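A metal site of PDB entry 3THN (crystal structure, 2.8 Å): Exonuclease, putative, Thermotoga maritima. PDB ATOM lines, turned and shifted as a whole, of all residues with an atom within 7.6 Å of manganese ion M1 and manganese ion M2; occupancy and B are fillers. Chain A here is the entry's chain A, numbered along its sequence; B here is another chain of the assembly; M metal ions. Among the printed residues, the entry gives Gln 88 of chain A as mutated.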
ATOM      1  N   SER A   7      30.061 -26.502 -16.071  1.00  0.00           N
ATOM      2  CA  SER A   7      28.782 -25.984 -15.618  1.00  0.00           C
ATOM      3  C   SER A   7      27.998 -26.980 -14.791  1.00  0.00           C
ATOM      4  O   SER A   7      28.317 -28.156 -14.753  1.00  0.00           O
ATOM      5  CB  SER A   7      27.957 -25.600 -16.853  1.00  0.00           C
ATOM      6  OG  SER A   7      27.076 -24.536 -16.554  1.00  0.00           O
ATOM      7  N   ASP A   8      26.952 -26.474 -14.148  1.00  0.00           N
ATOM      8  CA  ASP A   8      25.895 -27.334 -13.632  1.00  0.00           C
ATOM      9  C   ASP A   8      26.447 -28.424 -12.727  1.00  0.00           C
ATOM     10  O   ASP A   8      26.152 -29.605 -12.916  1.00  0.00           O
ATOM     11  CB  ASP A   8      25.100 -27.942 -14.794  1.00  0.00           C
ATOM     12  CG  ASP A   8      24.376 -26.884 -15.629  1.00  0.00           C
ATOM     13  OD1 ASP A   8      25.009 -26.333 -16.549  1.00  0.00           O
ATOM     14  OD2 ASP A   8      23.180 -26.624 -15.367  1.00  0.00           O
ATOM     15  N   TRP A   9      27.241 -28.015 -11.756  1.00  0.00           N
ATOM     16  CA  TRP A   9      27.889 -28.944 -10.848  1.00  0.00           C
ATOM     17  C   TRP A   9      26.893 -29.556  -9.873  1.00  0.00           C
ATOM     18  O   TRP A   9      26.941 -30.744  -9.578  1.00  0.00           O
ATOM     19  CB  TRP A   9      28.954 -28.220 -10.055  1.00  0.00           C
ATOM     20  CG  TRP A   9      30.125 -27.769 -10.854  1.00  0.00           C
ATOM     21  CD1 TRP A   9      30.408 -28.070 -12.156  1.00  0.00           C
ATOM     22  CD2 TRP A   9      31.192 -26.941 -10.381  1.00  0.00           C
ATOM     23  NE1 TRP A   9      31.597 -27.470 -12.521  1.00  0.00           N
ATOM     24  CE2 TRP A   9      32.095 -26.770 -11.454  1.00  0.00           C
ATOM     25  CE3 TRP A   9      31.476 -26.330  -9.163  1.00  0.00           C
ATOM     26  CZ2 TRP A   9      33.246 -26.006 -11.333  1.00  0.00           C
ATOM     27  CZ3 TRP A   9      32.626 -25.573  -9.049  1.00  0.00           C
ATOM     28  CH2 TRP A   9      33.498 -25.421 -10.132  1.00  0.00           C
ATOM     29  N   HIS A  10      25.998 -28.712  -9.369  1.00  0.00           N
ATOM     30  CA  HIS A  10      25.046 -29.121  -8.345  1.00  0.00           C
ATOM     31  C   HIS A  10      25.719 -29.639  -7.067  1.00  0.00           C
ATOM     32  O   HIS A  10      25.316 -30.664  -6.526  1.00  0.00           O
ATOM     33  CB  HIS A  10      24.079 -30.158  -8.886  1.00  0.00           C
ATOM     34  CG  HIS A  10      23.069 -29.593  -9.844  1.00  0.00           C
ATOM     35  ND1 HIS A  10      21.748 -29.425  -9.509  1.00  0.00           N
ATOM     36  CD2 HIS A  10      23.201 -29.146 -11.112  1.00  0.00           C
ATOM     37  CE1 HIS A  10      21.093 -28.903 -10.534  1.00  0.00           C
ATOM     38  NE2 HIS A  10      21.958 -28.727 -11.523  1.00  0.00           N
ATOM     39  N   THR A  50      29.340 -21.502 -16.059  1.00  0.00           N
ATOM     40  CA  THR A  50      28.032 -20.945 -16.442  1.00  0.00           C
ATOM     41  C   THR A  50      26.854 -21.313 -15.529  1.00  0.00           C
ATOM     42  O   THR A  50      25.738 -21.445 -16.001  1.00  0.00           O
ATOM     43  CB  THR A  50      27.680 -21.235 -17.918  1.00  0.00           C
ATOM     44  OG1 THR A  50      28.186 -22.522 -18.305  1.00  0.00           O
ATOM     45  CG2 THR A  50      28.296 -20.190 -18.830  1.00  0.00           C
ATOM     46  N   GLY A  51      27.103 -21.468 -14.235  1.00  0.00           N
ATOM     47  CA  GLY A  51      26.026 -21.443 -13.263  1.00  0.00           C
ATOM     48  C   GLY A  51      25.520 -22.779 -12.766  1.00  0.00           C
ATOM     49  O   GLY A  51      25.892 -23.817 -13.295  1.00  0.00           O
ATOM     50  N   ASP A  52      24.625 -22.729 -11.774  1.00  0.00           N
ATOM     51  CA  ASP A  52      24.125 -23.914 -11.053  1.00  0.00           C
ATOM     52  C   ASP A  52      25.263 -24.714 -10.427  1.00  0.00           C
ATOM     53  O   ASP A  52      25.245 -25.950 -10.436  1.00  0.00           O
ATOM     54  CB  ASP A  52      23.294 -24.820 -11.941  1.00  0.00           C
ATOM     55  CG  ASP A  52      21.917 -24.263 -12.232  1.00  0.00           C
ATOM     56  OD1 ASP A  52      21.516 -23.279 -11.565  1.00  0.00           O
ATOM     57  OD2 ASP A  52      21.243 -24.808 -13.140  1.00  0.00           O
ATOM     58  N   LEU A  53      26.250 -24.013  -9.883  1.00  0.00           N
ATOM     59  CA  LEU A  53      27.344 -24.667  -9.198  1.00  0.00           C
ATOM     60  C   LEU A  53      26.880 -25.308  -7.894  1.00  0.00           C
ATOM     61  O   LEU A  53      27.342 -26.384  -7.508  1.00  0.00           O
ATOM     62  CB  LEU A  53      28.450 -23.639  -8.929  1.00  0.00           C
ATOM     63  CG  LEU A  53      28.809 -22.871 -10.193  1.00  0.00           C
ATOM     64  CD1 LEU A  53      29.925 -21.915  -9.911  1.00  0.00           C
ATOM     65  CD2 LEU A  53      29.203 -23.842 -11.310  1.00  0.00           C
ATOM     66  N   LEU A  54      25.966 -24.630  -7.210  1.00  0.00           N
ATOM     67  CA  LEU A  54      25.329 -25.175  -6.024  1.00  0.00           C
ATOM     68  C   LEU A  54      23.980 -25.762  -6.381  1.00  0.00           C
ATOM     69  O   LEU A  54      23.384 -25.413  -7.410  1.00  0.00           O
ATOM     70  CB  LEU A  54      25.126 -24.104  -4.965  1.00  0.00           C
ATOM     71  CG  LEU A  54      26.315 -23.721  -4.112  1.00  0.00           C
ATOM     72  CD1 LEU A  54      25.919 -22.550  -3.233  1.00  0.00           C
ATOM     73  CD2 LEU A  54      26.720 -24.899  -3.282  1.00  0.00           C
ATOM     74  N   PRO A  85      26.298 -17.016 -12.238  1.00  0.00           N
ATOM     75  CA  PRO A  85      25.414 -17.879 -11.436  1.00  0.00           C
ATOM     76  C   PRO A  85      24.081 -18.130 -12.141  1.00  0.00           C
ATOM     77  O   PRO A  85      23.650 -17.292 -12.937  1.00  0.00           O
ATOM     78  CB  PRO A  85      25.213 -17.095 -10.138  1.00  0.00           C
ATOM     79  CG  PRO A  85      25.806 -15.726 -10.383  1.00  0.00           C
ATOM     80  CD  PRO A  85      26.824 -15.888 -11.462  1.00  0.00           C
ATOM     81  N   GLY A  86      23.462 -19.285 -11.875  1.00  0.00           N
ATOM     82  CA  GLY A  86      22.183 -19.666 -12.466  1.00  0.00           C
ATOM     83  C   GLY A  86      20.999 -19.554 -11.512  1.00  0.00           C
ATOM     84  O   GLY A  86      21.080 -18.912 -10.450  1.00  0.00           O
ATOM     85  N   ASN A  87      19.887 -20.189 -11.899  1.00  0.00           N
ATOM     86  CA  ASN A  87      18.654 -20.116 -11.122  1.00  0.00           C
ATOM     87  C   ASN A  87      18.792 -20.786  -9.764  1.00  0.00           C
ATOM     88  O   ASN A  87      18.245 -20.293  -8.789  1.00  0.00           O
ATOM     89  CB  ASN A  87      17.476 -20.729 -11.888  1.00  0.00           C
ATOM     90  CG  ASN A  87      17.849 -22.002 -12.620  1.00  0.00           C
ATOM     91  OD1 ASN A  87      18.774 -21.998 -13.455  1.00  0.00           O
ATOM     92  ND2 ASN A  87      17.184 -23.114 -12.294  1.00  0.00           N
ATOM     93  N   GLN A  88      19.537 -21.882  -9.701  1.00  0.00           N
ATOM     94  CA  GLN A  88      19.634 -22.674  -8.474  1.00  0.00           C
ATOM     95  C   GLN A  88      20.879 -22.399  -7.634  1.00  0.00           C
ATOM     96  O   GLN A  88      21.200 -23.173  -6.728  1.00  0.00           O
ATOM     97  CB  GLN A  88      19.597 -24.164  -8.780  1.00  0.00           C
ATOM     98  CG  GLN A  88      18.475 -24.552  -9.709  1.00  0.00           C
ATOM     99  CD  GLN A  88      18.613 -25.975 -10.172  1.00  0.00           C
ATOM    100  OE1 GLN A  88      19.040 -26.847  -9.400  1.00  0.00           O
ATOM    101  NE2 GLN A  88      18.285 -26.234 -11.451  1.00  0.00           N
ATOM    102  N   ASP A  89      21.605 -21.342  -7.924  1.00  0.00           N
ATOM    103  CA  ASP A  89      22.670 -20.957  -7.015  1.00  0.00           C
ATOM    104  C   ASP A  89      22.108 -20.106  -5.900  1.00  0.00           C
ATOM    105  O   ASP A  89      21.355 -19.155  -6.130  1.00  0.00           O
ATOM    106  CB  ASP A  89      23.782 -20.228  -7.760  1.00  0.00           C
ATOM    107  CG  ASP A  89      24.567 -21.149  -8.645  1.00  0.00           C
ATOM    108  OD1 ASP A  89      24.848 -20.766  -9.804  1.00  0.00           O
ATOM    109  OD2 ASP A  89      24.904 -22.264  -8.174  1.00  0.00           O
ATOM    110  N   TYR A 133      19.715 -16.166 -16.259  1.00  0.00           N
ATOM    111  CA  TYR A 133      18.443 -16.876 -16.362  1.00  0.00           C
ATOM    112  C   TYR A 133      17.268 -15.918 -16.422  1.00  0.00           C
ATOM    113  O   TYR A 133      17.143 -15.046 -15.571  1.00  0.00           O
ATOM    114  CB  TYR A 133      18.267 -17.819 -15.158  1.00  0.00           C
ATOM    115  CG  TYR A 133      17.129 -18.823 -15.258  1.00  0.00           C
ATOM    116  CD1 TYR A 133      17.142 -19.842 -16.207  1.00  0.00           C
ATOM    117  CD2 TYR A 133      16.072 -18.778 -14.351  1.00  0.00           C
ATOM    118  CE1 TYR A 133      16.106 -20.780 -16.274  1.00  0.00           C
ATOM    119  CE2 TYR A 133      15.030 -19.704 -14.414  1.00  0.00           C
ATOM    120  CZ  TYR A 133      15.054 -20.701 -15.367  1.00  0.00           C
ATOM    121  OH  TYR A 133      14.028 -21.612 -15.405  1.00  0.00           O
ATOM    122  N   HIS A 174      22.505 -18.534 -19.280  1.00  0.00           N
ATOM    123  CA  HIS A 174      21.975 -19.603 -18.454  1.00  0.00           C
ATOM    124  C   HIS A 174      20.484 -19.695 -18.746  1.00  0.00           C
ATOM    125  O   HIS A 174      19.694 -18.908 -18.220  1.00  0.00           O
ATOM    126  CB  HIS A 174      22.250 -19.348 -16.972  1.00  0.00           C
ATOM    127  CG  HIS A 174      22.014 -20.544 -16.100  1.00  0.00           C
ATOM    128  ND1 HIS A 174      23.024 -21.424 -15.766  1.00  0.00           N
ATOM    129  CD2 HIS A 174      20.891 -21.014 -15.512  1.00  0.00           C
ATOM    130  CE1 HIS A 174      22.527 -22.388 -15.004  1.00  0.00           C
ATOM    131  NE2 HIS A 174      21.230 -22.165 -14.845  1.00  0.00           N
ATOM    132  N   PHE A 175      20.126 -20.639 -19.625  1.00  0.00           N
ATOM    133  CA  PHE A 175      18.735 -20.816 -20.047  1.00  0.00           C
ATOM    134  C   PHE A 175      18.538 -22.065 -20.906  1.00  0.00           C
ATOM    135  O   PHE A 175      19.497 -22.761 -21.224  1.00  0.00           O
ATOM    136  CB  PHE A 175      18.242 -19.589 -20.820  1.00  0.00           C
ATOM    137  CG  PHE A 175      19.175 -19.142 -21.919  1.00  0.00           C
ATOM    138  CD1 PHE A 175      19.192 -19.799 -23.136  1.00  0.00           C
ATOM    139  CD2 PHE A 175      20.015 -18.051 -21.739  1.00  0.00           C
ATOM    140  CE1 PHE A 175      20.044 -19.392 -24.164  1.00  0.00           C
ATOM    141  CE2 PHE A 175      20.868 -17.639 -22.759  1.00  0.00           C
ATOM    142  CZ  PHE A 175      20.881 -18.318 -23.984  1.00  0.00           C
ATOM    143  N   THR A 176      17.292 -22.352 -21.260  1.00  0.00           N
ATOM    144  CA  THR A 176      17.007 -23.406 -22.225  1.00  0.00           C
ATOM    145  C   THR A 176      16.757 -22.812 -23.596  1.00  0.00           C
ATOM    146  O   THR A 176      16.034 -21.825 -23.719  1.00  0.00           O
ATOM    147  CB  THR A 176      15.764 -24.214 -21.856  1.00  0.00           C
ATOM    148  OG1 THR A 176      15.584 -24.192 -20.438  1.00  0.00           O
ATOM    149  CG2 THR A 176      15.910 -25.638 -22.356  1.00  0.00           C
ATOM    150  N   GLU A 191       9.211 -22.727 -18.730  1.00  0.00           N
ATOM    151  CA  GLU A 191      10.352 -21.822 -18.719  1.00  0.00           C
ATOM    152  C   GLU A 191      10.172 -20.789 -19.804  1.00  0.00           C
ATOM    153  O   GLU A 191       9.419 -21.024 -20.766  1.00  0.00           O
ATOM    154  CB  GLU A 191      11.647 -22.570 -19.023  1.00  0.00           C
ATOM    155  CG  GLU A 191      11.974 -23.725 -18.119  1.00  0.00           C
ATOM    156  CD  GLU A 191      13.447 -23.794 -17.823  1.00  0.00           C
ATOM    157  OE1 GLU A 191      14.136 -22.802 -18.139  1.00  0.00           O
ATOM    158  OE2 GLU A 191      13.917 -24.813 -17.269  1.00  0.00           O
ATOM    159  N   GLY A 209      24.704 -22.686 -19.825  1.00  0.00           N
ATOM    160  CA  GLY A 209      24.478 -23.616 -18.738  1.00  0.00           C
ATOM    161  C   GLY A 209      22.992 -23.708 -18.490  1.00  0.00           C
ATOM    162  O   GLY A 209      22.249 -22.841 -18.932  1.00  0.00           O
ATOM    163  N   HIS A 210      22.581 -24.790 -17.823  1.00  0.00           N
ATOM    164  CA  HIS A 210      21.241 -25.005 -17.253  1.00  0.00           C
ATOM    165  C   HIS A 210      20.761 -26.391 -17.690  1.00  0.00           C
ATOM    166  O   HIS A 210      20.015 -27.083 -16.994  1.00  0.00           O
ATOM    167  CB  HIS A 210      20.246 -23.917 -17.675  1.00  0.00           C
ATOM    168  CG  HIS A 210      18.828 -24.161 -17.227  1.00  0.00           C
ATOM    169  ND1 HIS A 210      18.413 -23.980 -15.930  1.00  0.00           N
ATOM    170  CD2 HIS A 210      17.733 -24.541 -17.929  1.00  0.00           C
ATOM    171  CE1 HIS A 210      17.120 -24.254 -15.836  1.00  0.00           C
ATOM    172  NE2 HIS A 210      16.690 -24.597 -17.038  1.00  0.00           N
ATOM    173  N   ILE A 211      21.238 -26.786 -18.852  1.00  0.00           N
ATOM    174  CA  ILE A 211      20.901 -28.066 -19.410  1.00  0.00           C
ATOM    175  C   ILE A 211      21.977 -29.049 -18.982  1.00  0.00           C
ATOM    176  O   ILE A 211      23.167 -28.712 -18.978  1.00  0.00           O
ATOM    177  CB  ILE A 211      20.729 -27.940 -20.947  1.00  0.00           C
ATOM    178  CG1 ILE A 211      19.424 -27.190 -21.220  1.00  0.00           C
ATOM    179  CG2 ILE A 211      20.708 -29.291 -21.609  1.00  0.00           C
ATOM    180  CD1 ILE A 211      18.216 -27.757 -20.483  1.00  0.00           C
ATOM    181  N   HIS A 212      21.559 -30.252 -18.584  1.00  0.00           N
ATOM    182  CA  HIS A 212      22.462 -31.239 -17.971  1.00  0.00           C
ATOM    183  C   HIS A 212      23.139 -32.149 -18.966  1.00  0.00           C
ATOM    184  O   HIS A 212      24.072 -32.870 -18.603  1.00  0.00           O
ATOM    185  CB  HIS A 212      21.725 -32.107 -16.943  1.00  0.00           C
ATOM    186  CG  HIS A 212      21.052 -31.332 -15.865  1.00  0.00           C
ATOM    187  ND1 HIS A 212      20.155 -31.889 -14.984  1.00  0.00           N
ATOM    188  CD2 HIS A 212      21.126 -30.017 -15.535  1.00  0.00           C
ATOM    189  CE1 HIS A 212      19.696 -30.960 -14.164  1.00  0.00           C
ATOM    190  NE2 HIS A 212      20.273 -29.810 -14.473  1.00  0.00           N
ATOM    191  N   GLY A 227      27.120 -29.741 -19.980  1.00  0.00           N
ATOM    192  CA  GLY A 227      26.382 -30.737 -19.217  1.00  0.00           C
ATOM    193  C   GLY A 227      26.794 -30.854 -17.764  1.00  0.00           C
ATOM    194  O   GLY A 227      27.712 -30.160 -17.320  1.00  0.00           O
ATOM    195  N   SER A 228      26.113 -31.719 -17.011  1.00  0.00           N
ATOM    196  CA  SER A 228      26.486 -32.016 -15.624  1.00  0.00           C
ATOM    197  C   SER A 228      27.798 -32.790 -15.604  1.00  0.00           C
ATOM    198  O   SER A 228      28.351 -33.120 -16.633  1.00  0.00           O
ATOM    199  CB  SER A 228      25.456 -32.892 -14.964  1.00  0.00           C
ATOM    200  OG  SER A 228      24.179 -32.683 -15.494  1.00  0.00           O
ATOM    201  N   ILE A 232      22.008 -36.959 -12.483  1.00  0.00           N
ATOM    202  CA  ILE A 232      21.260 -36.546 -11.291  1.00  0.00           C
ATOM    203  C   ILE A 232      20.031 -37.420 -10.975  1.00  0.00           C
ATOM    204  O   ILE A 232      19.899 -37.862  -9.833  1.00  0.00           O
ATOM    205  CB  ILE A 232      20.858 -35.047 -11.379  1.00  0.00           C
ATOM    206  CG1 ILE A 232      22.093 -34.168 -11.148  1.00  0.00           C
ATOM    207  CG2 ILE A 232      19.816 -34.729 -10.347  1.00  0.00           C
ATOM    208  CD1 ILE A 232      22.080 -32.852 -11.954  1.00  0.00           C
ATOM    209  N   ALA B 181      17.761 -32.004 -20.753  1.00  0.00           N
ATOM    210  CA  ALA B 181      17.288 -31.897 -19.377  1.00  0.00           C
ATOM    211  C   ALA B 181      18.338 -31.054 -18.655  1.00  0.00           C
ATOM    212  O   ALA B 181      19.445 -30.938 -19.152  1.00  0.00           O
ATOM    213  CB  ALA B 181      17.268 -33.243 -18.756  1.00  0.00           C
ATOM    214  N   GLY B 182      18.034 -30.470 -17.503  1.00  0.00           N
ATOM    215  CA  GLY B 182      16.723 -30.403 -16.926  1.00  0.00           C
ATOM    216  C   GLY B 182      16.076 -29.035 -17.138  1.00  0.00           C
ATOM    217  O   GLY B 182      16.311 -28.049 -16.415  1.00  0.00           O
HETATM  218 MN    MN M   1      19.748 -23.614 -14.229  1.00  0.00          MN
HETATM  219 MN    MN M   2      21.491 -27.293 -13.816  1.00  0.00          MN
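Along chain A the residues within 4 Å of manganese ion M1 span positions 52 to 210.
N of His 10 is in hydrogen-bond range of O of Leu 53 (3.3 Å).
OD1 of Asp 8 lies within hydrogen-bond range of OG of Ser 7 (2.7 Å).
The backbone NH of Gln 88 sits at hydrogen-bond distance from the side-chain carboxylate of Asp 52 (3.1 Å).
The backbone carbonyl oxygen (O) of Asp 52 is in hydrogen-bond range of the backbone NH (N) of Trp 9 (3.2 Å).
The backbone NH of Asp 52 sits at hydrogen-bond distance from the side-chain carboxylate of Asp 89 (2.8 Å).
The side-chain carboxylate (OE2) of Glu 191 sits at hydrogen-bond distance from a ring nitrogen (NE2) of His 210 (2.8 Å).
The backbone carbonyl oxygen (O) of Gly 51 is in hydrogen-bond range of the backbone NH (N) of Asp 8 (3.0 Å).
The backbone NH of Ser 228 lies within hydrogen-bond range of the backbone carbonyl oxygen of His 212, at 2.8 Å.
Within 4 Å of manganese ion M2: Asp 8, His 10, Asp 52, His 210 and His 212.
The nearest printed residue that does not touch manganese ion M2 is Gln 88 (4.1 Å).
Manganese ion M1 is bound by OD1 of Asn 87 (2.0 Å), NE2 of His 174 (2.2 Å), ND1 of His 210 (2.2 Å) and OD2 of Asp 52 (2.2 Å).
OD2 of Asp 8 binds manganese ion M2 (2.4 Å).
OD2 of Asp 52 binds manganese ion M2.
Slightly farther from manganese ion M2 lies a ring nitrogen (NE2) of His 10 (2.7 Å).
Slightly farther from manganese ion M2 lies NE2 of His 212 (2.9 Å).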
